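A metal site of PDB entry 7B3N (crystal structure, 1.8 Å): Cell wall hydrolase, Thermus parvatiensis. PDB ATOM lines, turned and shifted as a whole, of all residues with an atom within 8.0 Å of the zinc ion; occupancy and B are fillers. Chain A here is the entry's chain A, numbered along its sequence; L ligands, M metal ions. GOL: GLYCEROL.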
ATOM      1  N   PRO A  15      11.478 -20.162  -4.346  1.00  0.00           N
ATOM      2  CA  PRO A  15      10.217 -20.636  -4.948  1.00  0.00           C
ATOM      3  C   PRO A  15       9.034 -19.836  -4.397  1.00  0.00           C
ATOM      4  O   PRO A  15       8.775 -19.916  -3.221  1.00  0.00           O
ATOM      5  CB  PRO A  15      10.095 -22.077  -4.454  1.00  0.00           C
ATOM      6  CG  PRO A  15      11.464 -22.438  -3.948  1.00  0.00           C
ATOM      7  CD  PRO A  15      12.078 -21.173  -3.468  1.00  0.00           C
ATOM      8  N   GLY A  16       8.405 -19.051  -5.251  1.00  0.00           N
ATOM      9  CA  GLY A  16       7.298 -18.168  -4.833  1.00  0.00           C
ATOM     10  C   GLY A  16       6.168 -18.926  -4.162  1.00  0.00           C
ATOM     11  O   GLY A  16       5.895 -20.080  -4.503  1.00  0.00           O
ATOM     12  N   HIS A  17       5.493 -18.293  -3.218  1.00  0.00           N
ATOM     13  CA  HIS A  17       4.256 -18.831  -2.649  1.00  0.00           C
ATOM     14  C   HIS A  17       4.636 -20.017  -1.799  1.00  0.00           C
ATOM     15  O   HIS A  17       5.788 -20.050  -1.316  1.00  0.00           O
ATOM     16  CB  HIS A  17       3.265 -19.071  -3.789  1.00  0.00           C
ATOM     17  CG  HIS A  17       3.108 -17.908  -4.706  1.00  0.00           C
ATOM     18  ND1 HIS A  17       2.561 -16.697  -4.294  1.00  0.00           N
ATOM     19  CD2 HIS A  17       3.501 -17.720  -5.983  1.00  0.00           C
ATOM     20  CE1 HIS A  17       2.631 -15.842  -5.280  1.00  0.00           C
ATOM     21  NE2 HIS A  17       3.187 -16.447  -6.327  1.00  0.00           N
ATOM     22  N   ASP A  21      -0.586 -20.390   0.413  1.00  0.00           N
ATOM     23  CA  ASP A  21      -0.533 -19.521  -0.794  1.00  0.00           C
ATOM     24  C   ASP A  21      -0.212 -20.362  -2.017  1.00  0.00           C
ATOM     25  O   ASP A  21       0.958 -20.760  -2.218  1.00  0.00           O
ATOM     26  CB  ASP A  21       0.483 -18.395  -0.592  1.00  0.00           C
ATOM     27  CG  ASP A  21       0.583 -17.458  -1.775  1.00  0.00           C
ATOM     28  OD1 ASP A  21      -0.284 -17.563  -2.670  1.00  0.00           O
ATOM     29  OD2 ASP A  21       1.564 -16.671  -1.804  1.00  0.00           O
ATOM     30  N   PRO A  22      -1.201 -20.673  -2.884  1.00  0.00           N
ATOM     31  CA  PRO A  22      -0.929 -21.514  -4.049  1.00  0.00           C
ATOM     32  C   PRO A  22      -0.279 -20.781  -5.231  1.00  0.00           C
ATOM     33  O   PRO A  22       0.129 -21.427  -6.162  1.00  0.00           O
ATOM     34  CB  PRO A  22      -2.352 -22.023  -4.423  1.00  0.00           C
ATOM     35  CG  PRO A  22      -3.267 -20.870  -4.003  1.00  0.00           C
ATOM     36  CD  PRO A  22      -2.622 -20.295  -2.764  1.00  0.00           C
ATOM     37  N   GLY A  23      -0.279 -19.453  -5.179  1.00  0.00           N
ATOM     38  CA  GLY A  23       0.007 -18.603  -6.342  1.00  0.00           C
ATOM     39  C   GLY A  23      -1.110 -18.814  -7.349  1.00  0.00           C
ATOM     40  O   GLY A  23      -2.203 -19.122  -6.913  1.00  0.00           O
ATOM     41  N   ALA A  24      -0.818 -18.729  -8.631  1.00  0.00           N
ATOM     42  CA  ALA A  24      -1.816 -18.958  -9.708  1.00  0.00           C
ATOM     43  C   ALA A  24      -2.201 -20.447  -9.690  1.00  0.00           C
ATOM     44  O   ALA A  24      -1.325 -21.310  -9.352  1.00  0.00           O
ATOM     45  CB  ALA A  24      -1.230 -18.540 -11.035  1.00  0.00           C
ATOM     46  N   GLU A  32       0.856 -22.971  -8.976  1.00  0.00           N
ATOM     47  CA  GLU A  32       2.118 -22.241  -9.182  1.00  0.00           C
ATOM     48  C   GLU A  32       3.140 -22.610  -8.084  1.00  0.00           C
ATOM     49  O   GLU A  32       4.296 -22.895  -8.433  1.00  0.00           O
ATOM     50  CB  GLU A  32       1.867 -20.752  -9.170  1.00  0.00           C
ATOM     51  CG  GLU A  32       3.068 -19.986  -9.660  1.00  0.00           C
ATOM     52  CD  GLU A  32       3.087 -18.554  -9.235  1.00  0.00           C
ATOM     53  OE1 GLU A  32       1.957 -18.003  -9.009  1.00  0.00           O
ATOM     54  OE2 GLU A  32       4.219 -18.017  -9.068  1.00  0.00           O
ATOM     55  N   ALA A  33       2.719 -22.653  -6.811  1.00  0.00           N
ATOM     56  CA  ALA A  33       3.618 -22.944  -5.672  1.00  0.00           C
ATOM     57  C   ALA A  33       4.385 -24.241  -5.947  1.00  0.00           C
ATOM     58  O   ALA A  33       5.597 -24.266  -5.636  1.00  0.00           O
ATOM     59  CB  ALA A  33       2.828 -23.009  -4.391  1.00  0.00           C
ATOM     60  N   ASN A  36       6.841 -23.828  -8.870  1.00  0.00           N
ATOM     61  CA  ASN A  36       7.961 -22.997  -8.374  1.00  0.00           C
ATOM     62  C   ASN A  36       8.993 -23.862  -7.655  1.00  0.00           C
ATOM     63  O   ASN A  36      10.169 -23.722  -7.964  1.00  0.00           O
ATOM     64  CB  ASN A  36       7.473 -21.882  -7.456  1.00  0.00           C
ATOM     65  CG  ASN A  36       6.636 -20.881  -8.224  1.00  0.00           C
ATOM     66  OD1 ASN A  36       6.663 -20.853  -9.454  1.00  0.00           O
ATOM     67  ND2 ASN A  36       5.897 -20.042  -7.501  1.00  0.00           N
ATOM     68  N   SER A  83      14.157 -15.186  -7.427  1.00  0.00           N
ATOM     69  CA  SER A  83      12.805 -15.657  -7.153  1.00  0.00           C
ATOM     70  C   SER A  83      12.255 -16.407  -8.388  1.00  0.00           C
ATOM     71  O   SER A  83      12.440 -15.966  -9.568  1.00  0.00           O
ATOM     72  CB  SER A  83      11.980 -14.485  -6.697  1.00  0.00           C
ATOM     73  OG  SER A  83      10.739 -14.924  -6.238  1.00  0.00           O
ATOM     74  N   VAL A  84      11.610 -17.539  -8.122  1.00  0.00           N
ATOM     75  CA  VAL A  84      11.099 -18.493  -9.142  1.00  0.00           C
ATOM     76  C   VAL A  84       9.574 -18.479  -9.080  1.00  0.00           C
ATOM     77  O   VAL A  84       9.001 -18.923  -8.080  1.00  0.00           O
ATOM     78  CB  VAL A  84      11.694 -19.889  -8.936  1.00  0.00           C
ATOM     79  CG1 VAL A  84      11.075 -20.878  -9.908  1.00  0.00           C
ATOM     80  CG2 VAL A  84      13.208 -19.836  -9.107  1.00  0.00           C
ATOM     81  N   HIS A  85       8.944 -17.968 -10.129  1.00  0.00           N
ATOM     82  CA  HIS A  85       7.471 -17.874 -10.267  1.00  0.00           C
ATOM     83  C   HIS A  85       7.016 -18.354 -11.646  1.00  0.00           C
ATOM     84  O   HIS A  85       7.851 -18.632 -12.522  1.00  0.00           O
ATOM     85  CB  HIS A  85       6.982 -16.458 -10.055  1.00  0.00           C
ATOM     86  CG  HIS A  85       7.127 -15.943  -8.666  1.00  0.00           C
ATOM     87  ND1 HIS A  85       6.036 -15.684  -7.901  1.00  0.00           N
ATOM     88  CD2 HIS A  85       8.215 -15.610  -7.936  1.00  0.00           C
ATOM     89  CE1 HIS A  85       6.428 -15.231  -6.725  1.00  0.00           C
ATOM     90  NE2 HIS A  85       7.798 -15.191  -6.711  1.00  0.00           N
ATOM     91  N   HIS A  86       5.719 -18.643 -11.724  1.00  0.00           N
ATOM     92  CA  HIS A  86       5.003 -18.943 -12.990  1.00  0.00           C
ATOM     93  C   HIS A  86       3.842 -17.956 -13.078  1.00  0.00           C
ATOM     94  O   HIS A  86       3.396 -17.477 -12.041  1.00  0.00           O
ATOM     95  CB  HIS A  86       4.627 -20.411 -13.073  1.00  0.00           C
ATOM     96  CG  HIS A  86       5.803 -21.320 -13.189  1.00  0.00           C
ATOM     97  ND1 HIS A  86       6.531 -21.686 -12.083  1.00  0.00           N
ATOM     98  CD2 HIS A  86       6.332 -21.967 -14.241  1.00  0.00           C
ATOM     99  CE1 HIS A  86       7.522 -22.495 -12.472  1.00  0.00           C
ATOM    100  NE2 HIS A  86       7.387 -22.706 -13.789  1.00  0.00           N
ATOM    101  N   ASP A  87       3.486 -17.554 -14.294  1.00  0.00           N
ATOM    102  CA  ASP A  87       2.497 -16.470 -14.491  1.00  0.00           C
ATOM    103  C   ASP A  87       1.091 -17.068 -14.433  1.00  0.00           C
ATOM    104  O   ASP A  87       0.950 -18.307 -14.309  1.00  0.00           O
ATOM    105  CB  ASP A  87       2.831 -15.756 -15.794  1.00  0.00           C
ATOM    106  CG  ASP A  87       2.557 -14.273 -15.748  1.00  0.00           C
ATOM    107  OD1 ASP A  87       1.513 -13.885 -15.182  1.00  0.00           O
ATOM    108  OD2 ASP A  87       3.406 -13.518 -16.242  1.00  0.00           O
ATOM    109  N   THR A  88       0.069 -16.227 -14.565  1.00  0.00           N
ATOM    110  CA  THR A  88      -1.343 -16.672 -14.687  1.00  0.00           C
ATOM    111  C   THR A  88      -1.456 -17.679 -15.832  1.00  0.00           C
ATOM    112  O   THR A  88      -0.642 -17.668 -16.773  1.00  0.00           O
ATOM    113  CB  THR A  88      -2.267 -15.482 -14.964  1.00  0.00           C
ATOM    114  OG1 THR A  88      -1.904 -15.080 -16.285  1.00  0.00           O
ATOM    115  CG2 THR A  88      -2.072 -14.331 -14.003  1.00  0.00           C
ATOM    116  N   TYR A 133       8.781  -7.690  -3.300  1.00  0.00           N
ATOM    117  CA  TYR A 133       9.560  -8.006  -2.080  1.00  0.00           C
ATOM    118  C   TYR A 133      11.044  -8.171  -2.401  1.00  0.00           C
ATOM    119  O   TYR A 133      11.872  -7.936  -1.509  1.00  0.00           O
ATOM    120  CB  TYR A 133       8.989  -9.256  -1.422  1.00  0.00           C
ATOM    121  CG  TYR A 133       9.091 -10.579  -2.169  1.00  0.00           C
ATOM    122  CD1 TYR A 133       8.100 -10.970  -3.036  1.00  0.00           C
ATOM    123  CD2 TYR A 133      10.040 -11.520  -1.813  1.00  0.00           C
ATOM    124  CE1 TYR A 133       8.071 -12.245  -3.600  1.00  0.00           C
ATOM    125  CE2 TYR A 133      10.075 -12.778  -2.417  1.00  0.00           C
ATOM    126  CZ  TYR A 133       9.079 -13.155  -3.293  1.00  0.00           C
ATOM    127  OH  TYR A 133       8.989 -14.434  -3.786  1.00  0.00           O
ATOM    128  N   LEU A 143      12.993 -11.645 -10.197  1.00  0.00           N
ATOM    129  CA  LEU A 143      11.829 -12.559 -10.079  1.00  0.00           C
ATOM    130  C   LEU A 143      11.552 -13.068 -11.498  1.00  0.00           C
ATOM    131  O   LEU A 143      11.197 -12.261 -12.356  1.00  0.00           O
ATOM    132  CB  LEU A 143      10.656 -11.805  -9.439  1.00  0.00           C
ATOM    133  CG  LEU A 143       9.435 -12.641  -9.089  1.00  0.00           C
ATOM    134  CD1 LEU A 143       8.597 -11.980  -8.017  1.00  0.00           C
ATOM    135  CD2 LEU A 143       8.568 -12.928 -10.309  1.00  0.00           C
ATOM    136  N   VAL A 144      11.845 -14.324 -11.768  1.00  0.00           N
ATOM    137  CA  VAL A 144      11.669 -14.944 -13.092  1.00  0.00           C
ATOM    138  C   VAL A 144      10.257 -15.515 -13.175  1.00  0.00           C
ATOM    139  O   VAL A 144       9.862 -16.285 -12.247  1.00  0.00           O
ATOM    140  CB  VAL A 144      12.725 -16.005 -13.362  1.00  0.00           C
ATOM    141  CG1 VAL A 144      12.563 -16.582 -14.769  1.00  0.00           C
ATOM    142  CG2 VAL A 144      14.114 -15.441 -13.114  1.00  0.00           C
ATOM    143  N   GLU A 145       9.474 -15.058 -14.159  1.00  0.00           N
ATOM    144  CA  GLU A 145       8.151 -15.670 -14.479  1.00  0.00           C
ATOM    145  C   GLU A 145       8.437 -16.625 -15.637  1.00  0.00           C
ATOM    146  O   GLU A 145       8.688 -16.149 -16.757  1.00  0.00           O
ATOM    147  CB  GLU A 145       7.136 -14.624 -14.905  1.00  0.00           C
ATOM    148  CG  GLU A 145       6.738 -13.656 -13.830  1.00  0.00           C
ATOM    149  CD  GLU A 145       5.625 -14.207 -12.968  1.00  0.00           C
ATOM    150  OE1 GLU A 145       5.408 -15.419 -13.044  1.00  0.00           O
ATOM    151  OE2 GLU A 145       4.985 -13.426 -12.220  1.00  0.00           O
ATOM    152  N   THR A 149       1.276 -20.770 -15.537  1.00  0.00           N
ATOM    153  CA  THR A 149       0.954 -21.864 -14.604  1.00  0.00           C
ATOM    154  C   THR A 149       0.116 -22.892 -15.390  1.00  0.00           C
ATOM    155  O   THR A 149      -1.031 -22.562 -15.800  1.00  0.00           O
ATOM    156  CB  THR A 149       0.290 -21.339 -13.338  1.00  0.00           C
ATOM    157  OG1 THR A 149       1.216 -20.436 -12.699  1.00  0.00           O
ATOM    158  CG2 THR A 149      -0.116 -22.439 -12.391  1.00  0.00           C
HETATM  159  C1  GOL L   1       2.235 -12.207  -8.639  1.00  0.00           C
HETATM  160  O1  GOL L   1       2.764 -11.381  -7.603  1.00  0.00           O
HETATM  161  C2  GOL L   1       3.211 -13.281  -9.058  1.00  0.00           C
HETATM  162  O2  GOL L   1       3.485 -14.147  -7.965  1.00  0.00           O
HETATM  163  C3  GOL L   1       2.751 -14.091 -10.237  1.00  0.00           C
HETATM  164  O3  GOL L   1       3.545 -15.269 -10.435  1.00  0.00           O
HETATM  165 ZN    ZN M   1       4.019 -16.048  -8.320  1.00  0.00          ZN
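The nearest printed residue that does not touch the zinc ion is His 86 (4.03 Å).
The side-chain hydroxyl (OH) of Tyr 133 lies within hydrogen-bond range of a ring nitrogen (NE2) of His 85, at 3.2 Å. The backbone NH (N) of His 85 lies within hydrogen-bond range of the backbone carbonyl oxygen (O) of Val 144. A ring nitrogen (NE2) of His 85 is in hydrogen-bond range of the side-chain hydroxyl (OG) of Ser 83, at 3.0 Å. The side-chain carboxylate (OE2) of Glu 32 sits close to the backbone NH (N) of His 86 (3.1 Å). OD1 of Asn 36 lies close to O of Glu 32, 3.3 Å away. O of Ala 24 sits at hydrogen-bond distance from N of Glu 32, 2.8 Å away. The backbone NH of Glu 32 sits at hydrogen-bond distance from the backbone carbonyl oxygen of Pro 22. OD2 of Asp 21 is in hydrogen-bond range of ND1 of His 17, 2.7 Å away.
The zinc ion is bound by an oxygen (O2) of the ligand (2.0 Å). The zinc ion is bound by ND1 of His 85 (2.1 Å). OE2 of Glu 32 binds the zinc ion. NE2 of His 17 is bound to the zinc ion (2.2 Å). An oxygen (O3) of the ligand is bound to the zinc ion (2.3 Å). The zinc ion has five donor atoms within binding distance.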
